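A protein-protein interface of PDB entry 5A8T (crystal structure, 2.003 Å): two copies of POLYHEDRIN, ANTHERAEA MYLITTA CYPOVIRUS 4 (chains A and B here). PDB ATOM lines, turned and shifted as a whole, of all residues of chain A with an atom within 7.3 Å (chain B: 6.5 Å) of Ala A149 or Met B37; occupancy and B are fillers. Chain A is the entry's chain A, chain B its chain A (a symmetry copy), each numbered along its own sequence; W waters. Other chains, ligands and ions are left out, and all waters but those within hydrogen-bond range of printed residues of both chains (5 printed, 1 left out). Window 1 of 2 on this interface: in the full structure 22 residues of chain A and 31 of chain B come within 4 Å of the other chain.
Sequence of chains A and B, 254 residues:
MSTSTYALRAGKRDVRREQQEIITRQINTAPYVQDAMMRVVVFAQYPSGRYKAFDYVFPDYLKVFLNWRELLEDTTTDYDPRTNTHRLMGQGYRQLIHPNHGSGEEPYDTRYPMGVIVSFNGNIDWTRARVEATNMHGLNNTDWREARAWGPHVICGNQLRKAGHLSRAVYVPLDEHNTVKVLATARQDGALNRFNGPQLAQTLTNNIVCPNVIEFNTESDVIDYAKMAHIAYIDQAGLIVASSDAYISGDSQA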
ATOM      1  N   ARG A 130      21.516   1.735  23.577  1.00  0.00           N
ATOM      2  CA  ARG A 130      22.473   2.734  24.004  1.00  0.00           C
ATOM      3  C   ARG A 130      22.251   3.222  25.418  1.00  0.00           C
ATOM      4  O   ARG A 130      21.141   3.172  25.951  1.00  0.00           O
ATOM      5  CB  ARG A 130      22.438   3.929  23.054  1.00  0.00           C
ATOM      6  CG  ARG A 130      21.118   4.696  23.092  1.00  0.00           C
ATOM      7  CD  ARG A 130      21.044   5.697  21.943  1.00  0.00           C
ATOM      8  NE  ARG A 130      20.848   5.005  20.677  1.00  0.00           N
ATOM      9  CZ  ARG A 130      20.636   5.608  19.514  1.00  0.00           C
ATOM     10  NH1 ARG A 130      20.603   6.937  19.446  1.00  0.00           N
ATOM     11  NH2 ARG A 130      20.457   4.876  18.421  1.00  0.00           N
ATOM     12  N   GLU A 132      23.790   6.554  28.066  1.00  0.00           N
ATOM     13  CA  GLU A 132      24.696   7.673  28.261  1.00  0.00           C
ATOM     14  C   GLU A 132      24.489   8.288  29.630  1.00  0.00           C
ATOM     15  O   GLU A 132      23.394   8.222  30.191  1.00  0.00           O
ATOM     16  CB  GLU A 132      24.582   8.707  27.133  1.00  0.00           C
ATOM     17  CG  GLU A 132      23.633   9.861  27.373  1.00  0.00           C
ATOM     18  CD  GLU A 132      23.549  10.785  26.162  1.00  0.00           C
ATOM     19  OE1 GLU A 132      24.375  10.636  25.235  1.00  0.00           O
ATOM     20  OE2 GLU A 132      22.647  11.646  26.126  1.00  0.00           O
ATOM     21  N   THR A 134      24.369  11.653  31.522  1.00  0.00           N
ATOM     22  CA  THR A 134      24.179  13.068  31.251  1.00  0.00           C
ATOM     23  C   THR A 134      24.393  13.851  32.545  1.00  0.00           C
ATOM     24  O   THR A 134      24.653  13.252  33.592  1.00  0.00           O
ATOM     25  CB  THR A 134      22.782  13.316  30.639  1.00  0.00           C
ATOM     26  OG1 THR A 134      21.818  12.458  31.270  1.00  0.00           O
ATOM     27  CG2 THR A 134      22.799  12.995  29.144  1.00  0.00           C
ATOM     28  N   HIS A 137      20.784  17.790  34.697  1.00  0.00           N
ATOM     29  CA  HIS A 137      19.603  18.271  33.977  1.00  0.00           C
ATOM     30  C   HIS A 137      19.177  17.297  32.883  1.00  0.00           C
ATOM     31  O   HIS A 137      18.175  17.512  32.195  1.00  0.00           O
ATOM     32  CB  HIS A 137      19.872  19.652  33.378  1.00  0.00           C
ATOM     33  CG  HIS A 137      20.059  20.720  34.408  1.00  0.00           C
ATOM     34  ND1 HIS A 137      21.293  21.037  34.937  1.00  0.00           N
ATOM     35  CD2 HIS A 137      19.163  21.521  35.034  1.00  0.00           C
ATOM     36  CE1 HIS A 137      21.150  21.995  35.837  1.00  0.00           C
ATOM     37  NE2 HIS A 137      19.868  22.307  35.915  1.00  0.00           N
ATOM     38  N   GLY A 138      19.940  16.218  32.742  1.00  0.00           N
ATOM     39  CA  GLY A 138      19.757  15.295  31.643  1.00  0.00           C
ATOM     40  C   GLY A 138      20.317  15.796  30.322  1.00  0.00           C
ATOM     41  O   GLY A 138      19.862  15.376  29.255  1.00  0.00           O
ATOM     42  N   LEU A 139      21.312  16.677  30.379  1.00  0.00           N
ATOM     43  CA  LEU A 139      21.892  17.225  29.155  1.00  0.00           C
ATOM     44  C   LEU A 139      23.271  16.625  28.882  1.00  0.00           C
ATOM     45  O   LEU A 139      24.011  16.308  29.806  1.00  0.00           O
ATOM     46  CB  LEU A 139      21.984  18.758  29.236  1.00  0.00           C
ATOM     47  CG  LEU A 139      20.685  19.565  29.328  1.00  0.00           C
ATOM     48  CD1 LEU A 139      20.980  20.991  29.815  1.00  0.00           C
ATOM     49  CD2 LEU A 139      19.963  19.590  27.986  1.00  0.00           C
ATOM     50  N   ASN A 140      23.606  16.459  27.608  1.00  0.00           N
ATOM     51  CA  ASN A 140      24.927  15.955  27.237  1.00  0.00           C
ATOM     52  C   ASN A 140      25.882  17.064  26.795  1.00  0.00           C
ATOM     53  O   ASN A 140      26.966  16.790  26.290  1.00  0.00           O
ATOM     54  CB  ASN A 140      24.837  14.858  26.174  1.00  0.00           C
ATOM     55  CG  ASN A 140      23.910  15.224  25.031  1.00  0.00           C
ATOM     56  OD1 ASN A 140      23.867  16.368  24.588  1.00  0.00           O
ATOM     57  ND2 ASN A 140      23.159  14.248  24.550  1.00  0.00           N
ATOM     58  N   ASP A 143      25.596  23.542  28.108  1.00  0.00           N
ATOM     59  CA  ASP A 143      24.730  24.531  27.480  1.00  0.00           C
ATOM     60  C   ASP A 143      23.674  23.790  26.654  1.00  0.00           C
ATOM     61  O   ASP A 143      24.005  23.162  25.645  1.00  0.00           O
ATOM     62  CB  ASP A 143      25.575  25.435  26.578  1.00  0.00           C
ATOM     63  CG  ASP A 143      24.831  26.679  26.112  1.00  0.00           C
ATOM     64  OD1 ASP A 143      23.610  26.596  25.858  1.00  0.00           O
ATOM     65  OD2 ASP A 143      25.483  27.742  25.996  1.00  0.00           O
ATOM     66  N   TRP A 144      22.416  23.854  27.087  1.00  0.00           N
ATOM     67  CA  TRP A 144      21.356  23.099  26.436  1.00  0.00           C
ATOM     68  C   TRP A 144      21.244  23.432  24.960  1.00  0.00           C
ATOM     69  O   TRP A 144      20.871  22.576  24.170  1.00  0.00           O
ATOM     70  CB  TRP A 144      19.991  23.307  27.123  1.00  0.00           C
ATOM     71  CG  TRP A 144      19.368  24.671  26.900  1.00  0.00           C
ATOM     72  CD1 TRP A 144      19.482  25.763  27.712  1.00  0.00           C
ATOM     73  CD2 TRP A 144      18.529  25.072  25.809  1.00  0.00           C
ATOM     74  NE1 TRP A 144      18.778  26.819  27.193  1.00  0.00           N
ATOM     75  CE2 TRP A 144      18.186  26.424  26.023  1.00  0.00           C
ATOM     76  CE3 TRP A 144      18.036  24.421  24.667  1.00  0.00           C
ATOM     77  CZ2 TRP A 144      17.376  27.142  25.136  1.00  0.00           C
ATOM     78  CZ3 TRP A 144      17.244  25.140  23.783  1.00  0.00           C
ATOM     79  CH2 TRP A 144      16.919  26.488  24.025  1.00  0.00           C
ATOM     80  N   ARG A 145      21.569  24.674  24.599  1.00  0.00           N
ATOM     81  CA  ARG A 145      21.478  25.137  23.215  1.00  0.00           C
ATOM     82  C   ARG A 145      22.383  24.352  22.273  1.00  0.00           C
ATOM     83  O   ARG A 145      22.169  24.351  21.058  1.00  0.00           O
ATOM     84  CB  ARG A 145      21.801  26.632  23.118  1.00  0.00           C
ATOM     85  CG  ARG A 145      20.768  27.524  23.777  1.00  0.00           C
ATOM     86  CD  ARG A 145      21.280  28.952  23.925  1.00  0.00           C
ATOM     87  NE  ARG A 145      22.518  29.020  24.701  1.00  0.00           N
ATOM     88  CZ  ARG A 145      23.072  30.161  25.104  1.00  0.00           C
ATOM     89  NH1 ARG A 145      22.491  31.304  24.812  1.00  0.00           N
ATOM     90  NH2 ARG A 145      24.203  30.161  25.793  1.00  0.00           N
ATOM     91  N   GLU A 146      23.389  23.677  22.823  1.00  0.00           N
ATOM     92  CA  GLU A 146      24.227  22.818  21.989  1.00  0.00           C
ATOM     93  C   GLU A 146      24.122  21.340  22.379  1.00  0.00           C
ATOM     94  O   GLU A 146      24.948  20.517  21.981  1.00  0.00           O
ATOM     95  CB  GLU A 146      25.672  23.324  21.971  1.00  0.00           C
ATOM     96  CG  GLU A 146      25.737  24.772  21.484  1.00  0.00           C
ATOM     97  CD  GLU A 146      27.144  25.263  21.208  1.00  0.00           C
ATOM     98  OE1 GLU A 146      28.020  25.085  22.076  1.00  0.00           O
ATOM     99  OE2 GLU A 146      27.373  25.842  20.127  1.00  0.00           O
ATOM    100  N   ALA A 147      23.091  21.007  23.148  1.00  0.00           N
ATOM    101  CA  ALA A 147      22.853  19.624  23.517  1.00  0.00           C
ATOM    102  C   ALA A 147      21.950  18.966  22.483  1.00  0.00           C
ATOM    103  O   ALA A 147      21.297  19.647  21.690  1.00  0.00           O
ATOM    104  CB  ALA A 147      22.248  19.526  24.930  1.00  0.00           C
ATOM    105  N   ARG A 148      21.932  17.638  22.485  1.00  0.00           N
ATOM    106  CA  ARG A 148      21.172  16.863  21.512  1.00  0.00           C
ATOM    107  C   ARG A 148      20.548  15.658  22.189  1.00  0.00           C
ATOM    108  O   ARG A 148      20.873  15.347  23.333  1.00  0.00           O
ATOM    109  CB  ARG A 148      22.085  16.389  20.373  1.00  0.00           C
ATOM    110  CG  ARG A 148      22.189  17.364  19.202  1.00  0.00           C
ATOM    111  CD  ARG A 148      23.315  18.380  19.376  1.00  0.00           C
ATOM    112  NE  ARG A 148      23.354  19.270  18.218  1.00  0.00           N
ATOM    113  CZ  ARG A 148      22.770  20.463  18.159  1.00  0.00           C
ATOM    114  NH1 ARG A 148      22.114  20.945  19.210  1.00  0.00           N
ATOM    115  NH2 ARG A 148      22.847  21.176  17.040  1.00  0.00           N
ATOM    116  N   ALA A 149      19.664  14.971  21.476  1.00  0.00           N
ATOM    117  CA  ALA A 149      19.014  13.782  22.015  1.00  0.00           C
ATOM    118  C   ALA A 149      20.043  12.788  22.549  1.00  0.00           C
ATOM    119  O   ALA A 149      19.841  12.164  23.588  1.00  0.00           O
ATOM    120  CB  ALA A 149      18.129  13.128  20.951  1.00  0.00           C
ATOM    121  N   TRP A 150      21.147  12.640  21.832  1.00  0.00           N
ATOM    122  CA  TRP A 150      22.246  11.808  22.305  1.00  0.00           C
ATOM    123  C   TRP A 150      23.578  12.502  22.054  1.00  0.00           C
ATOM    124  O   TRP A 150      23.710  13.283  21.110  1.00  0.00           O
ATOM    125  CB  TRP A 150      22.199  10.430  21.639  1.00  0.00           C
ATOM    126  CG  TRP A 150      20.891   9.734  21.883  1.00  0.00           C
ATOM    127  CD1 TRP A 150      19.796   9.739  21.071  1.00  0.00           C
ATOM    128  CD2 TRP A 150      20.532   8.960  23.036  1.00  0.00           C
ATOM    129  NE1 TRP A 150      18.780   9.006  21.639  1.00  0.00           N
ATOM    130  CE2 TRP A 150      19.206   8.520  22.847  1.00  0.00           C
ATOM    131  CE3 TRP A 150      21.204   8.595  24.206  1.00  0.00           C
ATOM    132  CZ2 TRP A 150      18.543   7.724  23.780  1.00  0.00           C
ATOM    133  CZ3 TRP A 150      20.537   7.805  25.141  1.00  0.00           C
ATOM    134  CH2 TRP A 150      19.223   7.381  24.920  1.00  0.00           C
ATOM    135  N   GLY A 151      24.554  12.230  22.915  1.00  0.00           N
ATOM    136  CA  GLY A 151      25.867  12.839  22.798  1.00  0.00           C
ATOM    137  C   GLY A 151      26.719  12.158  21.744  1.00  0.00           C
ATOM    138  O   GLY A 151      26.381  11.080  21.278  1.00  0.00           O
ATOM    139  N   LYS A 181      20.552   7.831  30.987  1.00  0.00           N
ATOM    140  CA  LYS A 181      19.573   7.620  29.932  1.00  0.00           C
ATOM    141  C   LYS A 181      19.803   6.277  29.256  1.00  0.00           C
ATOM    142  O   LYS A 181      20.945   5.861  29.053  1.00  0.00           O
ATOM    143  CB  LYS A 181      19.629   8.752  28.905  1.00  0.00           C
ATOM    144  CG  LYS A 181      19.194  10.101  29.459  1.00  0.00           C
ATOM    145  CD  LYS A 181      19.707  11.244  28.597  1.00  0.00           C
ATOM    146  CE  LYS A 181      19.213  11.128  27.162  1.00  0.00           C
ATOM    147  NZ  LYS A 181      19.994  12.031  26.253  1.00  0.00           N
ATOM    148  N   ALA B  30      22.344  26.316  16.681  1.00  0.00           N
ATOM    149  CA  ALA B  30      22.414  24.913  17.059  1.00  0.00           C
ATOM    150  C   ALA B  30      21.059  24.338  17.496  1.00  0.00           C
ATOM    151  O   ALA B  30      20.768  23.182  17.224  1.00  0.00           O
ATOM    152  CB  ALA B  30      23.475  24.713  18.144  1.00  0.00           C
ATOM    153  N   PRO B  31      20.225  25.138  18.187  1.00  0.00           N
ATOM    154  CA  PRO B  31      18.916  24.580  18.555  1.00  0.00           C
ATOM    155  C   PRO B  31      17.988  24.233  17.368  1.00  0.00           C
ATOM    156  O   PRO B  31      16.985  23.553  17.576  1.00  0.00           O
ATOM    157  CB  PRO B  31      18.288  25.697  19.400  1.00  0.00           C
ATOM    158  CG  PRO B  31      19.446  26.426  19.979  1.00  0.00           C
ATOM    159  CD  PRO B  31      20.526  26.380  18.928  1.00  0.00           C
ATOM    160  N   VAL B  33      18.864  22.504  14.697  1.00  0.00           N
ATOM    161  CA  VAL B  33      19.228  21.223  14.100  1.00  0.00           C
ATOM    162  C   VAL B  33      18.216  20.155  14.540  1.00  0.00           C
ATOM    163  O   VAL B  33      17.672  20.213  15.644  1.00  0.00           O
ATOM    164  CB  VAL B  33      20.667  20.819  14.471  1.00  0.00           C
ATOM    165  CG1 VAL B  33      20.975  19.384  14.029  1.00  0.00           C
ATOM    166  CG2 VAL B  33      21.667  21.797  13.862  1.00  0.00           C
ATOM    167  N   ASP B  35      18.049  17.181  15.736  1.00  0.00           N
ATOM    168  CA  ASP B  35      18.102  16.439  16.997  1.00  0.00           C
ATOM    169  C   ASP B  35      18.492  17.318  18.189  1.00  0.00           C
ATOM    170  O   ASP B  35      18.941  16.818  19.219  1.00  0.00           O
ATOM    171  CB  ASP B  35      19.044  15.235  16.883  1.00  0.00           C
ATOM    172  CG  ASP B  35      20.497  15.643  16.731  1.00  0.00           C
ATOM    173  OD1 ASP B  35      20.755  16.721  16.158  1.00  0.00           O
ATOM    174  OD2 ASP B  35      21.384  14.891  17.195  1.00  0.00           O
ATOM    175  N   ALA B  36      18.314  18.626  18.040  1.00  0.00           N
ATOM    176  CA  ALA B  36      18.629  19.565  19.106  1.00  0.00           C
ATOM    177  C   ALA B  36      17.650  19.406  20.259  1.00  0.00           C
ATOM    178  O   ALA B  36      16.555  18.844  20.102  1.00  0.00           O
ATOM    179  CB  ALA B  36      18.583  20.983  18.582  1.00  0.00           C
ATOM    180  N   MET B  37      18.047  19.905  21.422  1.00  0.00           N
ATOM    181  CA  MET B  37      17.182  19.872  22.583  1.00  0.00           C
ATOM    182  C   MET B  37      16.336  21.136  22.637  1.00  0.00           C
ATOM    183  O   MET B  37      16.709  22.185  22.104  1.00  0.00           O
ATOM    184  CB  MET B  37      17.989  19.712  23.874  1.00  0.00           C
ATOM    185  CG  MET B  37      18.711  18.377  24.007  1.00  0.00           C
ATOM    186  SD  MET B  37      17.632  16.924  24.095  1.00  0.00           S
ATOM    187  CE  MET B  37      17.101  16.986  25.801  1.00  0.00           C
ATOM    188  N   MET B  38      15.181  21.007  23.270  1.00  0.00           N
ATOM    189  CA  MET B  38      14.316  22.127  23.552  1.00  0.00           C
ATOM    190  C   MET B  38      14.190  22.164  25.063  1.00  0.00           C
ATOM    191  O   MET B  38      14.479  21.182  25.743  1.00  0.00           O
ATOM    192  CB  MET B  38      12.943  21.925  22.900  1.00  0.00           C
ATOM    193  CG  MET B  38      12.927  22.123  21.384  1.00  0.00           C
ATOM    194  SD  MET B  38      11.352  21.654  20.624  1.00  0.00           S
ATOM    195  CE  MET B  38      11.521  19.868  20.669  1.00  0.00           C
ATOM    196  N   ARG B  39      13.775  23.292  25.608  1.00  0.00           N
ATOM    197  CA  ARG B  39      13.681  23.390  27.052  1.00  0.00           C
ATOM    198  C   ARG B  39      12.452  24.186  27.428  1.00  0.00           C
ATOM    199  O   ARG B  39      12.325  25.340  27.039  1.00  0.00           O
ATOM    200  CB  ARG B  39      14.950  24.029  27.628  1.00  0.00           C
ATOM    201  CG  ARG B  39      15.056  23.980  29.166  1.00  0.00           C
ATOM    202  CD  ARG B  39      16.482  24.295  29.592  1.00  0.00           C
ATOM    203  NE  ARG B  39      16.738  24.017  30.992  1.00  0.00           N
ATOM    204  CZ  ARG B  39      17.949  24.023  31.536  1.00  0.00           C
ATOM    205  NH1 ARG B  39      19.013  24.279  30.783  1.00  0.00           N
ATOM    206  NH2 ARG B  39      18.104  23.758  32.827  1.00  0.00           N
ATOM    207  N   VAL B  57      13.785  19.174  29.637  1.00  0.00           N
ATOM    208  CA  VAL B  57      14.550  19.184  28.390  1.00  0.00           C
ATOM    209  C   VAL B  57      14.140  17.964  27.550  1.00  0.00           C
ATOM    210  O   VAL B  57      13.945  16.883  28.089  1.00  0.00           O
ATOM    211  CB  VAL B  57      16.085  19.278  28.633  1.00  0.00           C
ATOM    212  CG1 VAL B  57      16.409  20.548  29.374  1.00  0.00           C
ATOM    213  CG2 VAL B  57      16.596  18.091  29.434  1.00  0.00           C
ATOM    214  N   PHE B  58      13.948  18.159  26.246  1.00  0.00           N
ATOM    215  CA  PHE B  58      13.415  17.118  25.356  1.00  0.00           C
ATOM    216  C   PHE B  58      13.761  17.477  23.922  1.00  0.00           C
ATOM    217  O   PHE B  58      13.871  18.653  23.597  1.00  0.00           O
ATOM    218  CB  PHE B  58      11.885  17.049  25.477  1.00  0.00           C
ATOM    219  CG  PHE B  58      11.194  18.358  25.160  1.00  0.00           C
ATOM    220  CD1 PHE B  58      11.179  19.395  26.089  1.00  0.00           C
ATOM    221  CD2 PHE B  58      10.581  18.557  23.935  1.00  0.00           C
ATOM    222  CE1 PHE B  58      10.555  20.597  25.806  1.00  0.00           C
ATOM    223  CE2 PHE B  58       9.953  19.758  23.642  1.00  0.00           C
ATOM    224  CZ  PHE B  58       9.941  20.780  24.579  1.00  0.00           C
ATOM    225  N   PRO B  59      13.915  16.472  23.052  1.00  0.00           N
ATOM    226  CA  PRO B  59      14.281  16.752  21.662  1.00  0.00           C
ATOM    227  C   PRO B  59      13.130  16.897  20.669  1.00  0.00           C
ATOM    228  O   PRO B  59      13.357  17.506  19.625  1.00  0.00           O
ATOM    229  CB  PRO B  59      15.135  15.536  21.283  1.00  0.00           C
ATOM    230  CG  PRO B  59      14.551  14.443  22.082  1.00  0.00           C
ATOM    231  CD  PRO B  59      14.134  15.058  23.399  1.00  0.00           C
ATOM    232  N   ASP B  60      11.939  16.375  20.954  1.00  0.00           N
ATOM    233  CA  ASP B  60      10.894  16.355  19.923  1.00  0.00           C
ATOM    234  C   ASP B  60       9.542  16.934  20.328  1.00  0.00           C
ATOM    235  O   ASP B  60       8.964  17.729  19.600  1.00  0.00           O
ATOM    236  CB  ASP B  60      10.709  14.935  19.382  1.00  0.00           C
ATOM    237  CG  ASP B  60      11.965  14.402  18.742  1.00  0.00           C
ATOM    238  OD1 ASP B  60      12.440  15.027  17.763  1.00  0.00           O
ATOM    239  OD2 ASP B  60      12.485  13.373  19.235  1.00  0.00           O
ATOM    240  N   ASN B 121      11.425  27.360  25.076  1.00  0.00           N
ATOM    241  CA  ASN B 121      12.744  27.675  24.521  1.00  0.00           C
ATOM    242  C   ASN B 121      13.212  26.659  23.489  1.00  0.00           C
ATOM    243  O   ASN B 121      13.143  25.448  23.708  1.00  0.00           O
ATOM    244  CB  ASN B 121      13.791  27.804  25.639  1.00  0.00           C
ATOM    245  CG  ASN B 121      13.365  28.775  26.741  1.00  0.00           C
ATOM    246  OD1 ASN B 121      13.629  29.974  26.668  1.00  0.00           O
ATOM    247  ND2 ASN B 121      12.723  28.253  27.770  1.00  0.00           N
ATOM    248  N   GLY B 122      13.680  27.157  22.355  1.00  0.00           N
ATOM    249  CA  GLY B 122      14.164  26.293  21.299  1.00  0.00           C
ATOM    250  C   GLY B 122      13.386  26.427  20.010  1.00  0.00           C
ATOM    251  O   GLY B 122      12.611  27.367  19.821  1.00  0.00           O
ATOM    252  N   ASN B 123      13.605  25.465  19.118  1.00  0.00           N
ATOM    253  CA  ASN B 123      12.988  25.443  17.805  1.00  0.00           C
ATOM    254  C   ASN B 123      11.568  24.910  17.909  1.00  0.00           C
ATOM    255  O   ASN B 123      11.212  23.916  17.298  1.00  0.00           O
ATOM    256  CB  ASN B 123      13.822  24.565  16.876  1.00  0.00           C
ATOM    257  CG  ASN B 123      13.322  24.571  15.454  1.00  0.00           C
ATOM    258  OD1 ASN B 123      12.649  25.499  15.024  1.00  0.00           O
ATOM    259  ND2 ASN B 123      13.665  23.528  14.708  1.00  0.00           N
ATOM    260  N   ASN B 206      13.153   8.274  20.260  1.00  0.00           N
ATOM    261  CA  ASN B 206      14.241   9.146  20.699  1.00  0.00           C
ATOM    262  C   ASN B 206      13.814  10.253  21.647  1.00  0.00           C
ATOM    263  O   ASN B 206      14.658  10.920  22.245  1.00  0.00           O
ATOM    264  CB  ASN B 206      14.950   9.773  19.498  1.00  0.00           C
ATOM    265  CG  ASN B 206      16.063   8.904  18.967  1.00  0.00           C
ATOM    266  OD1 ASN B 206      16.781   8.267  19.734  1.00  0.00           O
ATOM    267  ND2 ASN B 206      16.210   8.865  17.649  1.00  0.00           N
ATOM    268  N   ASN B 207      12.509  10.456  21.780  1.00  0.00           N
ATOM    269  CA  ASN B 207      12.008  11.533  22.623  1.00  0.00           C
ATOM    270  C   ASN B 207      12.001  11.192  24.112  1.00  0.00           C
ATOM    271  O   ASN B 207      10.972  10.823  24.678  1.00  0.00           O
ATOM    272  CB  ASN B 207      10.620  11.988  22.165  1.00  0.00           C
ATOM    273  CG  ASN B 207      10.197  13.284  22.819  1.00  0.00           C
ATOM    274  OD1 ASN B 207      10.758  14.348  22.535  1.00  0.00           O
ATOM    275  ND2 ASN B 207       9.213  13.206  23.706  1.00  0.00           N
ATOM    276  N   ILE B 208      13.160  11.328  24.744  1.00  0.00           N
ATOM    277  CA  ILE B 208      13.269  11.116  26.177  1.00  0.00           C
ATOM    278  C   ILE B 208      13.179  12.457  26.869  1.00  0.00           C
ATOM    279  O   ILE B 208      14.082  13.285  26.752  1.00  0.00           O
ATOM    280  CB  ILE B 208      14.596  10.430  26.571  1.00  0.00           C
ATOM    281  CG1 ILE B 208      14.709   9.066  25.894  1.00  0.00           C
ATOM    282  CG2 ILE B 208      14.679  10.275  28.083  1.00  0.00           C
ATOM    283  CD1 ILE B 208      15.942   8.294  26.306  1.00  0.00           C
ATOM    284  N   CYS B 210      13.363  14.775  30.002  1.00  0.00           N
ATOM    285  CA  CYS B 210      14.167  14.748  31.219  1.00  0.00           C
ATOM    286  C   CYS B 210      13.727  15.868  32.136  1.00  0.00           C
ATOM    287  O   CYS B 210      14.151  17.008  31.956  1.00  0.00           O
ATOM    288  CB  CYS B 210      15.648  14.932  30.869  1.00  0.00           C
ATOM    289  SG  CYS B 210      16.260  13.708  29.700  1.00  0.00           S
HETATM  290  O   HOH W   1      18.979  14.171  27.310  1.00  0.00           O
HETATM  291  O   HOH W   2      16.972  11.634  24.025  1.00  0.00           O
HETATM  292  O   HOH W   3      21.925  25.209  29.714  1.00  0.00           O
HETATM  293  O   HOH W   4      23.226  17.221  15.677  1.00  0.00           O
HETATM  294  O   HOH W   5      15.965  18.612  33.348  1.00  0.00           O
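The backbone NH (N) of Met B37 sits at hydrogen-bond distance from the backbone carbonyl oxygen (O) of Ala A147. The guanidinium group of Arg A148 is in hydrogen-bond range of the backbone carbonyl oxygen of Ala B30, 2.9 Å away. The backbone carbonyl oxygen (O) of Asp B35 is in hydrogen-bond range of the backbone NH (N) of Ala A149, 3.0 Å away. The indole nitrogen (NE1) of Trp A150 sits at hydrogen-bond distance from the side-chain amide oxygen (OD1) of Asn B206, at 2.9 Å. O of Arg A148 lies close to SD of Met B37 (3.7 Å).
The side-chain amide nitrogen of Asn A140 lies within hydrogen-bond range of the backbone carbonyl oxygen of Arg A148, at 2.8 Å. The side-chain carboxylate (OD2) of Asp A143 is in salt-bridge range of the guanidinium group (NH2) of Arg A145. NZ of Lys A181 sits at hydrogen-bond distance from O of Ala A149 (2.7 Å). N of Arg B39 sits at hydrogen-bond distance from O of Asn B121. The backbone carbonyl oxygen of Val B57 lies within hydrogen-bond range of the backbone NH of Cys B210 (2.9 Å). O of Ile B208 sits at hydrogen-bond distance from SG of Cys B210.
CD2 of His A137 touches NH2 of Arg B39, at 3.3 Å. CG2 of Val B57 touches O of His A137, 3.2 Å away. His A137 touches Cys B210. SG of Cys B210 touches O of Gly A138 (3.99 Å). Arg B39 touches Leu A139 (NH1 to CD1, 3.95 Å). Val B57 touches Leu A139. Ala B36 touches Ala A147 (CA to O, 3.7 Å). Asp B35 touches Arg A148 (O to CA, 3.2 Å). Ala B36 touches Arg A148 (CB to NH1, 3.6 Å). Pro B59 touches Ala A149 (CB to CB, 3.9 Å).
Of chain A, only Trp A144, Ala A147, Arg A148 and Ala A149 come within 4 Å of Met B37. Printed residues of chain A within 4 Å of Asn B121: Trp A144 (3.7 Å). Printed residues of chain B within 4 Å of Arg A148: Ala B30 (2.9 Å), Val B33 (3.4 Å), Asp B35 (3.2 Å), Ala B36 (3.6 Å) and Met B37 (3.6 Å). Of the printed residues of chain A, Arg B39 touches His A137 (3.3 Å), Leu A139 (3.95 Å) and Trp A144 (3.4 Å). Of the printed residues of chain A, Ile B208 touches Trp A150. Of the printed residues of chain B, Leu A139 touches Arg B39 (3.95 Å) and Val B57 (3.9 Å). Asn B123 touches none of the printed residues of chain A.
Hydrophobic or aromatic side chains of chain B within 4 Å of the printed part of chain A: Ala B30, Pro B31, Val B33, Ala B36, Met B37, Val B57, Pro B59 and Ile B208. Along chain B the printed residues that touch a printed residue of chain A span positions 30 to 210. Of the 17 printed residues of chain A, 9 touch a printed residue of chain B. Hydrophobic or aromatic side chains of chain A within 4 Å of the printed part of chain B: His A137, Leu A139, Trp A144, Ala A147, Ala A149 and Trp A150. Among the printed residues, no Asp or Glu carboxylate lies within 4 Å of a Lys or Arg side-chain nitrogen of the other chain.
No position is printed for both chains. Of the 24 pairs that touch across the chains among the printed residues, none has its exchanged pair printed and touching as well.
Water W1 lies within hydrogen-bond range of O of Gly A138 (2.5 Å), NZ of Lys A181 (2.6 Å) and SG of Cys B210 (3.6 Å). Water W4 lies within hydrogen-bond range of the side-chain carboxylate (OD1) of Asp B35 (2.6 Å) and the guanidinium group (NE) of Arg A148 (3.3 Å). Water W5 bridges the backbone carbonyl oxygen (O) of His A137 (2.7 Å) and the backbone carbonyl oxygen (O) of Cys B210 (2.8 Å). Water W2 bridges O of Ala A149 (3.0 Å) and O of Asn B206 (3.0 Å). Water W3 lies within hydrogen-bond range of the backbone NH of Trp A144 and the guanidinium group of Arg B39.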
